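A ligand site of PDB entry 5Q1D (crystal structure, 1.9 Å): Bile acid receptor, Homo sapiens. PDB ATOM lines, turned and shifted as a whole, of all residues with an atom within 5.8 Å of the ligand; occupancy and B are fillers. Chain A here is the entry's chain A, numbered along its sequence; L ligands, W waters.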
ATOM      1  N   PRO A  27     -31.240 -23.064   1.784  1.00  0.00           N
ATOM      2  CA  PRO A  27     -29.760 -23.160   1.882  1.00  0.00           C
ATOM      3  C   PRO A  27     -29.193 -24.389   1.184  1.00  0.00           C
ATOM      4  O   PRO A  27     -28.157 -24.286   0.537  1.00  0.00           O
ATOM      5  CB  PRO A  27     -29.511 -23.215   3.385  1.00  0.00           C
ATOM      6  CG  PRO A  27     -30.686 -22.515   3.980  1.00  0.00           C
ATOM      7  CD  PRO A  27     -31.850 -22.932   3.119  1.00  0.00           C
ATOM      8  N   ILE A  30     -28.339 -24.094  -2.732  1.00  0.00           N
ATOM      9  CA  ILE A  30     -27.111 -23.345  -2.952  1.00  0.00           C
ATOM     10  C   ILE A  30     -25.865 -24.201  -2.666  1.00  0.00           C
ATOM     11  O   ILE A  30     -25.002 -24.321  -3.531  1.00  0.00           O
ATOM     12  CB  ILE A  30     -27.217 -22.062  -2.042  1.00  0.00           C
ATOM     13  CG1 ILE A  30     -28.575 -21.339  -2.333  1.00  0.00           C
ATOM     14  CG2 ILE A  30     -26.023 -21.132  -2.215  1.00  0.00           C
ATOM     15  CD1 ILE A  30     -29.238 -20.648  -1.176  1.00  0.00           C
ATOM     16  N   THR A  31     -25.801 -24.824  -1.477  1.00  0.00           N
ATOM     17  CA  THR A  31     -24.657 -25.642  -1.048  1.00  0.00           C
ATOM     18  C   THR A  31     -24.515 -26.908  -1.867  1.00  0.00           C
ATOM     19  O   THR A  31     -23.394 -27.282  -2.180  1.00  0.00           O
ATOM     20  CB  THR A  31     -24.693 -25.923   0.447  1.00  0.00           C
ATOM     21  OG1 THR A  31     -25.900 -26.590   0.781  1.00  0.00           O
ATOM     22  CG2 THR A  31     -24.571 -24.640   1.255  1.00  0.00           C
ATOM     23  N   ILE A  34     -22.708 -25.832  -5.190  1.00  0.00           N
ATOM     24  CA  ILE A  34     -21.295 -25.520  -4.953  1.00  0.00           C
ATOM     25  C   ILE A  34     -20.508 -26.803  -4.665  1.00  0.00           C
ATOM     26  O   ILE A  34     -19.406 -26.980  -5.196  1.00  0.00           O
ATOM     27  CB  ILE A  34     -21.138 -24.446  -3.821  1.00  0.00           C
ATOM     28  CG1 ILE A  34     -21.914 -23.144  -4.133  1.00  0.00           C
ATOM     29  CG2 ILE A  34     -19.648 -24.136  -3.530  1.00  0.00           C
ATOM     30  CD1 ILE A  34     -22.203 -22.224  -2.912  1.00  0.00           C
ATOM     31  N   ASN A  44     -18.817 -19.137 -11.737  1.00  0.00           N
ATOM     32  CA  ASN A  44     -19.129 -18.690 -10.379  1.00  0.00           C
ATOM     33  C   ASN A  44     -19.584 -17.233 -10.318  1.00  0.00           C
ATOM     34  O   ASN A  44     -20.438 -16.895  -9.508  1.00  0.00           O
ATOM     35  CB  ASN A  44     -17.950 -18.918  -9.431  1.00  0.00           C
ATOM     36  CG  ASN A  44     -17.754 -20.365  -9.046  1.00  0.00           C
ATOM     37  OD1 ASN A  44     -18.716 -21.093  -8.799  1.00  0.00           O
ATOM     38  ND2 ASN A  44     -16.509 -20.769  -8.890  1.00  0.00           N
ATOM     39  N   PHE A  45     -19.043 -16.364 -11.206  1.00  0.00           N
ATOM     40  CA  PHE A  45     -19.486 -14.958 -11.232  1.00  0.00           C
ATOM     41  C   PHE A  45     -20.967 -14.897 -11.642  1.00  0.00           C
ATOM     42  O   PHE A  45     -21.740 -14.142 -11.051  1.00  0.00           O
ATOM     43  CB  PHE A  45     -18.627 -14.125 -12.189  1.00  0.00           C
ATOM     44  CG  PHE A  45     -18.998 -12.662 -12.156  1.00  0.00           C
ATOM     45  CD1 PHE A  45     -18.561 -11.840 -11.126  1.00  0.00           C
ATOM     46  CD2 PHE A  45     -19.805 -12.099 -13.145  1.00  0.00           C
ATOM     47  CE1 PHE A  45     -18.920 -10.487 -11.083  1.00  0.00           C
ATOM     48  CE2 PHE A  45     -20.150 -10.761 -13.113  1.00  0.00           C
ATOM     49  CZ  PHE A  45     -19.713  -9.962 -12.078  1.00  0.00           C
ATOM     50  N   ILE A  47     -23.175 -17.439 -11.371  1.00  0.00           N
ATOM     51  CA  ILE A  47     -23.981 -18.078 -10.320  1.00  0.00           C
ATOM     52  C   ILE A  47     -24.257 -16.984  -9.263  1.00  0.00           C
ATOM     53  O   ILE A  47     -25.392 -16.836  -8.813  1.00  0.00           O
ATOM     54  CB  ILE A  47     -23.281 -19.335  -9.706  1.00  0.00           C
ATOM     55  CG1 ILE A  47     -23.204 -20.496 -10.730  1.00  0.00           C
ATOM     56  CG2 ILE A  47     -24.011 -19.804  -8.417  1.00  0.00           C
ATOM     57  CD1 ILE A  47     -22.103 -21.526 -10.442  1.00  0.00           C
ATOM     58  N   LEU A  48     -23.235 -16.194  -8.925  1.00  0.00           N
ATOM     59  CA  LEU A  48     -23.377 -15.099  -7.939  1.00  0.00           C
ATOM     60  C   LEU A  48     -24.402 -14.054  -8.354  1.00  0.00           C
ATOM     61  O   LEU A  48     -25.235 -13.672  -7.531  1.00  0.00           O
ATOM     62  CB  LEU A  48     -22.016 -14.451  -7.609  1.00  0.00           C
ATOM     63  CG  LEU A  48     -22.010 -13.191  -6.694  1.00  0.00           C
ATOM     64  CD1 LEU A  48     -22.331 -13.523  -5.235  1.00  0.00           C
ATOM     65  CD2 LEU A  48     -20.700 -12.485  -6.776  1.00  0.00           C
ATOM     66  N   MET A  51     -27.933 -15.453  -8.170  1.00  0.00           N
ATOM     67  CA  MET A  51     -28.315 -15.631  -6.757  1.00  0.00           C
ATOM     68  C   MET A  51     -28.660 -14.286  -6.120  1.00  0.00           C
ATOM     69  O   MET A  51     -29.568 -14.215  -5.311  1.00  0.00           O
ATOM     70  CB  MET A  51     -27.150 -16.227  -5.955  1.00  0.00           C
ATOM     71  CG  MET A  51     -26.967 -17.725  -6.145  1.00  0.00           C
ATOM     72  SD  MET A  51     -28.227 -18.760  -5.371  1.00  0.00           S
ATOM     73  CE  MET A  51     -28.073 -18.242  -3.759  1.00  0.00           C
ATOM     74  N   ALA A  52     -27.889 -13.248  -6.445  1.00  0.00           N
ATOM     75  CA  ALA A  52     -28.065 -11.919  -5.865  1.00  0.00           C
ATOM     76  C   ALA A  52     -29.285 -11.233  -6.431  1.00  0.00           C
ATOM     77  O   ALA A  52     -29.923 -10.480  -5.700  1.00  0.00           O
ATOM     78  CB  ALA A  52     -26.822 -11.089  -6.115  1.00  0.00           C
ATOM     79  N   HIS A  55     -32.190 -12.940  -4.707  1.00  0.00           N
ATOM     80  CA  HIS A  55     -32.187 -12.481  -3.325  1.00  0.00           C
ATOM     81  C   HIS A  55     -32.790 -11.087  -3.151  1.00  0.00           C
ATOM     82  O   HIS A  55     -33.573 -10.894  -2.209  1.00  0.00           O
ATOM     83  CB  HIS A  55     -30.782 -12.523  -2.748  1.00  0.00           C
ATOM     84  CG  HIS A  55     -30.686 -11.986  -1.365  1.00  0.00           C
ATOM     85  ND1 HIS A  55     -30.287 -10.675  -1.142  1.00  0.00           N
ATOM     86  CD2 HIS A  55     -30.958 -12.564  -0.172  1.00  0.00           C
ATOM     87  CE1 HIS A  55     -30.341 -10.500   0.174  1.00  0.00           C
ATOM     88  NE2 HIS A  55     -30.731 -11.607   0.800  1.00  0.00           N
ATOM     89  N   MET A  89     -27.653  -9.624   1.966  1.00  0.00           N
ATOM     90  CA  MET A  89     -27.050 -10.714   1.202  1.00  0.00           C
ATOM     91  C   MET A  89     -25.949 -11.409   2.005  1.00  0.00           C
ATOM     92  O   MET A  89     -25.906 -12.644   2.036  1.00  0.00           O
ATOM     93  CB  MET A  89     -26.513 -10.231  -0.150  1.00  0.00           C
ATOM     94  CG  MET A  89     -25.731 -11.328  -0.884  1.00  0.00           C
ATOM     95  SD  MET A  89     -24.827 -10.796  -2.327  1.00  0.00           S
ATOM     96  CE  MET A  89     -23.610  -9.785  -1.554  1.00  0.00           C
ATOM     97  N   PHE A  90     -25.058 -10.639   2.650  1.00  0.00           N
ATOM     98  CA  PHE A  90     -23.981 -11.214   3.445  1.00  0.00           C
ATOM     99  C   PHE A  90     -24.500 -11.923   4.688  1.00  0.00           C
ATOM    100  O   PHE A  90     -23.865 -12.889   5.154  1.00  0.00           O
ATOM    101  CB  PHE A  90     -22.870 -10.200   3.803  1.00  0.00           C
ATOM    102  CG  PHE A  90     -21.931  -9.934   2.649  1.00  0.00           C
ATOM    103  CD1 PHE A  90     -20.999 -10.886   2.235  1.00  0.00           C
ATOM    104  CD2 PHE A  90     -22.050  -8.781   1.887  1.00  0.00           C
ATOM    105  CE1 PHE A  90     -20.184 -10.668   1.126  1.00  0.00           C
ATOM    106  CE2 PHE A  90     -21.216  -8.556   0.792  1.00  0.00           C
ATOM    107  CZ  PHE A  90     -20.279  -9.497   0.437  1.00  0.00           C
ATOM    108  N   ARG A  92     -27.409 -13.473   4.904  1.00  0.00           N
ATOM    109  CA  ARG A  92     -28.025 -14.696   4.410  1.00  0.00           C
ATOM    110  C   ARG A  92     -26.944 -15.697   4.008  1.00  0.00           C
ATOM    111  O   ARG A  92     -27.091 -16.900   4.258  1.00  0.00           O
ATOM    112  CB  ARG A  92     -28.984 -14.389   3.247  1.00  0.00           C
ATOM    113  CG  ARG A  92     -29.615 -15.668   2.646  1.00  0.00           C
ATOM    114  CD  ARG A  92     -30.475 -16.429   3.666  1.00  0.00           C
ATOM    115  NE  ARG A  92     -31.177 -17.522   3.018  1.00  0.00           N
ATOM    116  CZ  ARG A  92     -32.053 -18.325   3.610  1.00  0.00           C
ATOM    117  NH1 ARG A  92     -32.352 -18.165   4.889  1.00  0.00           N
ATOM    118  NH2 ARG A  92     -32.642 -19.293   2.921  1.00  0.00           N
ATOM    119  N   SER A  93     -25.831 -15.193   3.449  1.00  0.00           N
ATOM    120  CA  SER A  93     -24.667 -16.025   3.080  1.00  0.00           C
ATOM    121  C   SER A  93     -24.028 -16.636   4.319  1.00  0.00           C
ATOM    122  O   SER A  93     -23.620 -17.802   4.296  1.00  0.00           O
ATOM    123  CB  SER A  93     -23.627 -15.211   2.317  1.00  0.00           C
ATOM    124  OG  SER A  93     -24.108 -14.900   1.021  1.00  0.00           O
ATOM    125  N   ALA A  94     -23.958 -15.859   5.423  1.00  0.00           N
ATOM    126  CA  ALA A  94     -23.461 -16.311   6.726  1.00  0.00           C
ATOM    127  C   ALA A  94     -24.383 -17.379   7.305  1.00  0.00           C
ATOM    128  O   ALA A  94     -23.880 -18.343   7.879  1.00  0.00           O
ATOM    129  CB  ALA A  94     -23.364 -15.135   7.683  1.00  0.00           C
ATOM    130  N   ILE A  96     -26.407 -19.439   5.528  1.00  0.00           N
ATOM    131  CA  ILE A  96     -26.191 -20.617   4.669  1.00  0.00           C
ATOM    132  C   ILE A  96     -24.887 -21.295   5.050  1.00  0.00           C
ATOM    133  O   ILE A  96     -24.839 -22.534   5.190  1.00  0.00           O
ATOM    134  CB  ILE A  96     -26.214 -20.203   3.172  1.00  0.00           C
ATOM    135  CG1 ILE A  96     -27.602 -19.646   2.748  1.00  0.00           C
ATOM    136  CG2 ILE A  96     -25.790 -21.361   2.254  1.00  0.00           C
ATOM    137  CD1 ILE A  96     -27.606 -18.815   1.476  1.00  0.00           C
ATOM    138  N   PHE A  97     -23.808 -20.512   5.219  1.00  0.00           N
ATOM    139  CA  PHE A  97     -22.486 -21.067   5.553  1.00  0.00           C
ATOM    140  C   PHE A  97     -22.450 -21.848   6.863  1.00  0.00           C
ATOM    141  O   PHE A  97     -21.704 -22.815   6.980  1.00  0.00           O
ATOM    142  CB  PHE A  97     -21.397 -19.969   5.568  1.00  0.00           C
ATOM    143  CG  PHE A  97     -19.997 -20.529   5.738  1.00  0.00           C
ATOM    144  CD1 PHE A  97     -19.405 -21.251   4.710  1.00  0.00           C
ATOM    145  CD2 PHE A  97     -19.305 -20.378   6.932  1.00  0.00           C
ATOM    146  CE1 PHE A  97     -18.133 -21.809   4.886  1.00  0.00           C
ATOM    147  CE2 PHE A  97     -18.020 -20.903   7.088  1.00  0.00           C
ATOM    148  CZ  PHE A  97     -17.446 -21.619   6.074  1.00  0.00           C
ATOM    149  N   ASN A  98     -23.241 -21.417   7.846  1.00  0.00           N
ATOM    150  CA  ASN A  98     -23.250 -22.022   9.178  1.00  0.00           C
ATOM    151  C   ASN A  98     -24.284 -23.129   9.383  1.00  0.00           C
ATOM    152  O   ASN A  98     -24.379 -23.651  10.493  1.00  0.00           O
ATOM    153  CB  ASN A  98     -23.389 -20.929  10.218  1.00  0.00           C
ATOM    154  CG  ASN A  98     -22.112 -20.145  10.352  1.00  0.00           C
ATOM    155  OD1 ASN A  98     -21.091 -20.661  10.785  1.00  0.00           O
ATOM    156  ND2 ASN A  98     -22.134 -18.908   9.899  1.00  0.00           N
ATOM    157  N   LEU A 109     -16.898 -26.734   1.051  1.00  0.00           N
ATOM    158  CA  LEU A 109     -17.704 -25.564   0.723  1.00  0.00           C
ATOM    159  C   LEU A 109     -16.856 -24.292   0.848  1.00  0.00           C
ATOM    160  O   LEU A 109     -16.847 -23.480  -0.068  1.00  0.00           O
ATOM    161  CB  LEU A 109     -18.956 -25.495   1.595  1.00  0.00           C
ATOM    162  CG  LEU A 109     -19.917 -24.308   1.343  1.00  0.00           C
ATOM    163  CD1 LEU A 109     -20.716 -24.488   0.042  1.00  0.00           C
ATOM    164  CD2 LEU A 109     -20.846 -24.128   2.503  1.00  0.00           C
ATOM    165  N   ARG A 112     -14.097 -24.231  -1.888  1.00  0.00           N
ATOM    166  CA  ARG A 112     -14.699 -23.897  -3.179  1.00  0.00           C
ATOM    167  C   ARG A 112     -14.993 -22.410  -3.253  1.00  0.00           C
ATOM    168  O   ARG A 112     -14.706 -21.796  -4.273  1.00  0.00           O
ATOM    169  CB  ARG A 112     -15.962 -24.728  -3.442  1.00  0.00           C
ATOM    170  CG  ARG A 112     -15.661 -26.185  -3.751  1.00  0.00           C
ATOM    171  CD  ARG A 112     -15.914 -26.546  -5.191  1.00  0.00           C
ATOM    172  NE  ARG A 112     -15.331 -27.854  -5.513  1.00  0.00           N
ATOM    173  CZ  ARG A 112     -16.012 -28.990  -5.524  1.00  0.00           C
ATOM    174  NH1 ARG A 112     -17.312 -29.006  -5.268  1.00  0.00           N
ATOM    175  NH2 ARG A 112     -15.404 -30.130  -5.821  1.00  0.00           N
ATOM    176  N   ILE A 113     -15.503 -21.796  -2.165  1.00  0.00           N
ATOM    177  CA  ILE A 113     -15.773 -20.349  -2.124  1.00  0.00           C
ATOM    178  C   ILE A 113     -14.455 -19.541  -2.175  1.00  0.00           C
ATOM    179  O   ILE A 113     -14.393 -18.559  -2.913  1.00  0.00           O
ATOM    180  CB  ILE A 113     -16.721 -19.931  -0.966  1.00  0.00           C
ATOM    181  CG1 ILE A 113     -18.096 -20.614  -1.119  1.00  0.00           C
ATOM    182  CG2 ILE A 113     -16.897 -18.414  -0.891  1.00  0.00           C
ATOM    183  CD1 ILE A 113     -18.891 -20.722   0.162  1.00  0.00           C
ATOM    184  N   SER A 116     -13.413 -19.306  -5.837  1.00  0.00           N
ATOM    185  CA  SER A 116     -14.512 -18.971  -6.746  1.00  0.00           C
ATOM    186  C   SER A 116     -14.189 -17.839  -7.738  1.00  0.00           C
ATOM    187  O   SER A 116     -14.925 -17.677  -8.714  1.00  0.00           O
ATOM    188  CB  SER A 116     -15.776 -18.657  -5.958  1.00  0.00           C
ATOM    189  OG  SER A 116     -15.601 -17.520  -5.126  1.00  0.00           O
ATOM    190  N   ILE A 118     -13.189 -14.614  -6.401  1.00  0.00           N
ATOM    191  CA  ILE A 118     -13.135 -13.474  -5.497  1.00  0.00           C
ATOM    192  C   ILE A 118     -11.664 -13.190  -5.154  1.00  0.00           C
ATOM    193  O   ILE A 118     -10.883 -14.124  -4.973  1.00  0.00           O
ATOM    194  CB  ILE A 118     -14.024 -13.718  -4.251  1.00  0.00           C
ATOM    195  CG1 ILE A 118     -13.944 -12.550  -3.254  1.00  0.00           C
ATOM    196  CG2 ILE A 118     -13.702 -15.073  -3.579  1.00  0.00           C
ATOM    197  CD1 ILE A 118     -15.170 -12.366  -2.409  1.00  0.00           C
ATOM    198  N   MET A 126     -14.562 -11.966   4.989  1.00  0.00           N
ATOM    199  CA  MET A 126     -15.851 -12.605   4.730  1.00  0.00           C
ATOM    200  C   MET A 126     -16.024 -13.837   5.604  1.00  0.00           C
ATOM    201  O   MET A 126     -17.040 -13.949   6.291  1.00  0.00           O
ATOM    202  CB  MET A 126     -15.938 -12.982   3.256  1.00  0.00           C
ATOM    203  CG  MET A 126     -17.126 -12.446   2.568  1.00  0.00           C
ATOM    204  SD  MET A 126     -17.097 -12.909   0.824  1.00  0.00           S
ATOM    205  CE  MET A 126     -17.350 -14.611   0.931  1.00  0.00           C
ATOM    206  N   PHE A 127     -15.031 -14.741   5.590  1.00  0.00           N
ATOM    207  CA  PHE A 127     -15.046 -15.957   6.404  1.00  0.00           C
ATOM    208  C   PHE A 127     -14.836 -15.656   7.874  1.00  0.00           C
ATOM    209  O   PHE A 127     -15.283 -16.432   8.712  1.00  0.00           O
ATOM    210  CB  PHE A 127     -14.060 -17.016   5.881  1.00  0.00           C
ATOM    211  CG  PHE A 127     -14.621 -17.750   4.690  1.00  0.00           C
ATOM    212  CD1 PHE A 127     -15.718 -18.596   4.821  1.00  0.00           C
ATOM    213  CD2 PHE A 127     -14.075 -17.574   3.427  1.00  0.00           C
ATOM    214  CE1 PHE A 127     -16.264 -19.246   3.715  1.00  0.00           C
ATOM    215  CE2 PHE A 127     -14.607 -18.244   2.327  1.00  0.00           C
ATOM    216  CZ  PHE A 127     -15.696 -19.074   2.476  1.00  0.00           C
ATOM    217  N   TYR A 130     -18.396 -14.787   8.712  1.00  0.00           N
ATOM    218  CA  TYR A 130     -19.184 -16.011   8.716  1.00  0.00           C
ATOM    219  C   TYR A 130     -18.917 -16.876   9.949  1.00  0.00           C
ATOM    220  O   TYR A 130     -19.864 -17.393  10.535  1.00  0.00           O
ATOM    221  CB  TYR A 130     -18.946 -16.858   7.461  1.00  0.00           C
ATOM    222  CG  TYR A 130     -19.306 -16.224   6.134  1.00  0.00           C
ATOM    223  CD1 TYR A 130     -20.162 -15.124   6.074  1.00  0.00           C
ATOM    224  CD2 TYR A 130     -18.882 -16.789   4.941  1.00  0.00           C
ATOM    225  CE1 TYR A 130     -20.542 -14.580   4.860  1.00  0.00           C
ATOM    226  CE2 TYR A 130     -19.254 -16.243   3.714  1.00  0.00           C
ATOM    227  CZ  TYR A 130     -20.073 -15.128   3.683  1.00  0.00           C
ATOM    228  OH  TYR A 130     -20.442 -14.555   2.489  1.00  0.00           O
ATOM    229  N   MET A 211     -15.023  -5.459  -4.527  1.00  0.00           N
ATOM    230  CA  MET A 211     -15.030  -6.917  -4.321  1.00  0.00           C
ATOM    231  C   MET A 211     -15.510  -7.595  -5.604  1.00  0.00           C
ATOM    232  O   MET A 211     -14.907  -8.587  -6.038  1.00  0.00           O
ATOM    233  CB  MET A 211     -15.975  -7.263  -3.148  1.00  0.00           C
ATOM    234  CG  MET A 211     -15.797  -8.648  -2.582  1.00  0.00           C
ATOM    235  SD  MET A 211     -16.957  -9.099  -1.238  1.00  0.00           S
ATOM    236  CE  MET A 211     -16.576  -7.849  -0.015  1.00  0.00           C
ATOM    237  N   LEU A 212     -16.581  -7.052  -6.216  1.00  0.00           N
ATOM    238  CA  LEU A 212     -17.179  -7.594  -7.448  1.00  0.00           C
ATOM    239  C   LEU A 212     -16.343  -7.325  -8.692  1.00  0.00           C
ATOM    240  O   LEU A 212     -16.266  -8.195  -9.557  1.00  0.00           O
ATOM    241  CB  LEU A 212     -18.568  -7.028  -7.670  1.00  0.00           C
ATOM    242  CG  LEU A 212     -19.594  -7.279  -6.585  1.00  0.00           C
ATOM    243  CD1 LEU A 212     -20.593  -6.182  -6.562  1.00  0.00           C
ATOM    244  CD2 LEU A 212     -20.237  -8.640  -6.752  1.00  0.00           C
ATOM    245  N   TRP A 215     -13.182  -9.565  -9.072  1.00  0.00           N
ATOM    246  CA  TRP A 215     -13.441 -10.968  -9.411  1.00  0.00           C
ATOM    247  C   TRP A 215     -12.648 -11.320 -10.660  1.00  0.00           C
ATOM    248  O   TRP A 215     -12.673 -10.547 -11.623  1.00  0.00           O
ATOM    249  CB  TRP A 215     -14.926 -11.194  -9.659  1.00  0.00           C
ATOM    250  CG  TRP A 215     -15.369 -12.603  -9.448  1.00  0.00           C
ATOM    251  CD1 TRP A 215     -15.180 -13.661 -10.290  1.00  0.00           C
ATOM    252  CD2 TRP A 215     -16.060 -13.119  -8.306  1.00  0.00           C
ATOM    253  NE1 TRP A 215     -15.738 -14.798  -9.752  1.00  0.00           N
ATOM    254  CE2 TRP A 215     -16.280 -14.495  -8.534  1.00  0.00           C
ATOM    255  CE3 TRP A 215     -16.552 -12.547  -7.116  1.00  0.00           C
ATOM    256  CZ2 TRP A 215     -16.931 -15.317  -7.603  1.00  0.00           C
ATOM    257  CZ3 TRP A 215     -17.190 -13.360  -6.200  1.00  0.00           C
ATOM    258  CH2 TRP A 215     -17.380 -14.728  -6.450  1.00  0.00           C
HETATM  259  N1  LIG L   1     -21.800 -16.998  -1.504  1.00  0.00           N
HETATM  260  N2  LIG L   1     -20.825 -16.447   0.450  1.00  0.00           N
HETATM  261  C1  LIG L   1     -22.024 -18.077  -0.633  1.00  0.00           C
HETATM  262  C2  LIG L   1     -21.403 -17.712   0.570  1.00  0.00           C
HETATM  263  C3  LIG L   1     -23.767 -16.775  -2.983  1.00  0.00           C
HETATM  264  C4  LIG L   1     -22.234 -16.844  -2.913  1.00  0.00           C
HETATM  265  C5  LIG L   1     -22.666 -19.274  -0.818  1.00  0.00           C
HETATM  266  C6  LIG L   1     -22.104 -19.805   1.462  1.00  0.00           C
HETATM  267  C7  LIG L   1     -21.581 -17.864  -3.866  1.00  0.00           C
HETATM  268  C8  LIG L   1     -19.428 -14.556  -1.953  1.00  0.00           C
HETATM  269  C9  LIG L   1     -25.641 -15.594  -1.865  1.00  0.00           C
HETATM  270  C10 LIG L   1     -20.034 -12.315  -2.480  1.00  0.00           C
HETATM  271  C11 LIG L   1     -19.099 -13.330  -2.509  1.00  0.00           C
HETATM  272  C12 LIG L   1     -20.068 -17.979  -3.600  1.00  0.00           C
HETATM  273  C13 LIG L   1     -26.430 -16.390  -1.053  1.00  0.00           C
HETATM  274  F1  LIG L   1     -22.173 -20.690   2.463  1.00  0.00           F
HETATM  275  C14 LIG L   1     -21.451 -18.597   1.656  1.00  0.00           C
HETATM  276  C15 LIG L   1     -21.088 -16.068  -0.795  1.00  0.00           C
HETATM  277  C16 LIG L   1     -20.681 -14.776  -1.372  1.00  0.00           C
HETATM  278  C17 LIG L   1     -21.599 -13.733  -1.372  1.00  0.00           C
HETATM  279  C18 LIG L   1     -21.281 -12.498  -1.924  1.00  0.00           C
HETATM  280 CL1  LIG L   1     -19.647 -10.769  -3.163  1.00  0.00          CL
HETATM  281  C19 LIG L   1     -21.797 -17.486  -5.340  1.00  0.00           C
HETATM  282  C20 LIG L   1     -21.161 -18.505  -6.287  1.00  0.00           C
HETATM  283  C21 LIG L   1     -19.659 -18.660  -6.008  1.00  0.00           C
HETATM  284  C22 LIG L   1     -19.395 -19.003  -4.530  1.00  0.00           C
HETATM  285  O1  LIG L   1     -24.422 -17.443  -3.776  1.00  0.00           O
HETATM  286  N3  LIG L   1     -24.294 -15.913  -2.087  1.00  0.00           N
HETATM  287  C23 LIG L   1     -26.181 -14.462  -2.473  1.00  0.00           C
HETATM  288  C24 LIG L   1     -27.515 -14.138  -2.249  1.00  0.00           C
HETATM  289  C25 LIG L   1     -28.304 -14.934  -1.438  1.00  0.00           C
HETATM  290  C26 LIG L   1     -27.767 -16.056  -0.838  1.00  0.00           C
HETATM  291  C27 LIG L   1     -22.692 -20.129   0.253  1.00  0.00           C
HETATM  292  F2  LIG L   1     -23.324 -21.308   0.121  1.00  0.00           F
HETATM  293  O   HOH W   1     -31.404 -16.069  -1.275  1.00  0.00           O
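OG of Ser 93 is in hydrogen-bond range of N3 of the ligand (3.3 Å).
OH of Tyr 130 sits at hydrogen-bond distance from N2 of the ligand, at 2.8 Å.
The backbone carbonyl oxygen (O) of Ser 116 is in hydrogen-bond range of the indole nitrogen (NE1) of Trp 215 (3.2 Å).
OG of Ser 93 sits at hydrogen-bond distance from O of Met 89 (3.1 Å).
The side-chain amide nitrogen (ND2) of Asn 44 lies close to the backbone carbonyl oxygen (O) of Ser 116 (3.5 Å).
The side-chain hydroxyl of Thr 31 sits at hydrogen-bond distance from the backbone carbonyl oxygen of Pro 27, 3.2 Å away.
The side-chain amide nitrogen (ND2) of Asn 98 is in hydrogen-bond range of the backbone carbonyl oxygen (O) of Tyr 130.
The backbone carbonyl oxygen (O) of Ile 34 is in hydrogen-bond range of the guanidinium group (NH1) of Arg 112, 2.9 Å away.
The backbone carbonyl oxygen (O) of Ile 113 is in hydrogen-bond range of the side-chain hydroxyl (OG) of Ser 116.
The backbone NH (N) of Phe 97 lies close to a fluorine (F1) of the ligand (3.2 Å).
CG2 of Ile 30 touches F2 of the ligand (3.6 Å).
CG2 of Thr 31 touches F2 of the ligand (3.7 Å).
Ile 34 touches the ligand.
O of Asn 44 touches C20 of the ligand, 3.7 Å away.
Ile 47 touches the ligand.
Leu 48 touches the ligand (CD1 to C18, 3.6 Å).
CG of Met 51 touches O1 of the ligand, 3.5 Å away.
His 55 touches the ligand (CB to C24, 3.7 Å).
CG of Met 89 touches C23 of the ligand, at 3.5 Å.
CE1 of Phe 90 touches C18 of the ligand, at 3.7 Å.
Arg 92 touches the ligand (CG to C26, 3.96 Å).
Ile 96 touches the ligand.
CD2 of Leu 109 touches F1 of the ligand, at 3.7 Å.
CD1 of Ile 113 touches C6 of the ligand (3.6 Å).
Ser 116 touches the ligand.
Met 126 touches the ligand (CE to C8, 3.6 Å).
Met 211 touches the ligand (SD to CL1, 3.7 Å).
Of the 30 residues printed, 20 come within 4 Å of the ligand.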
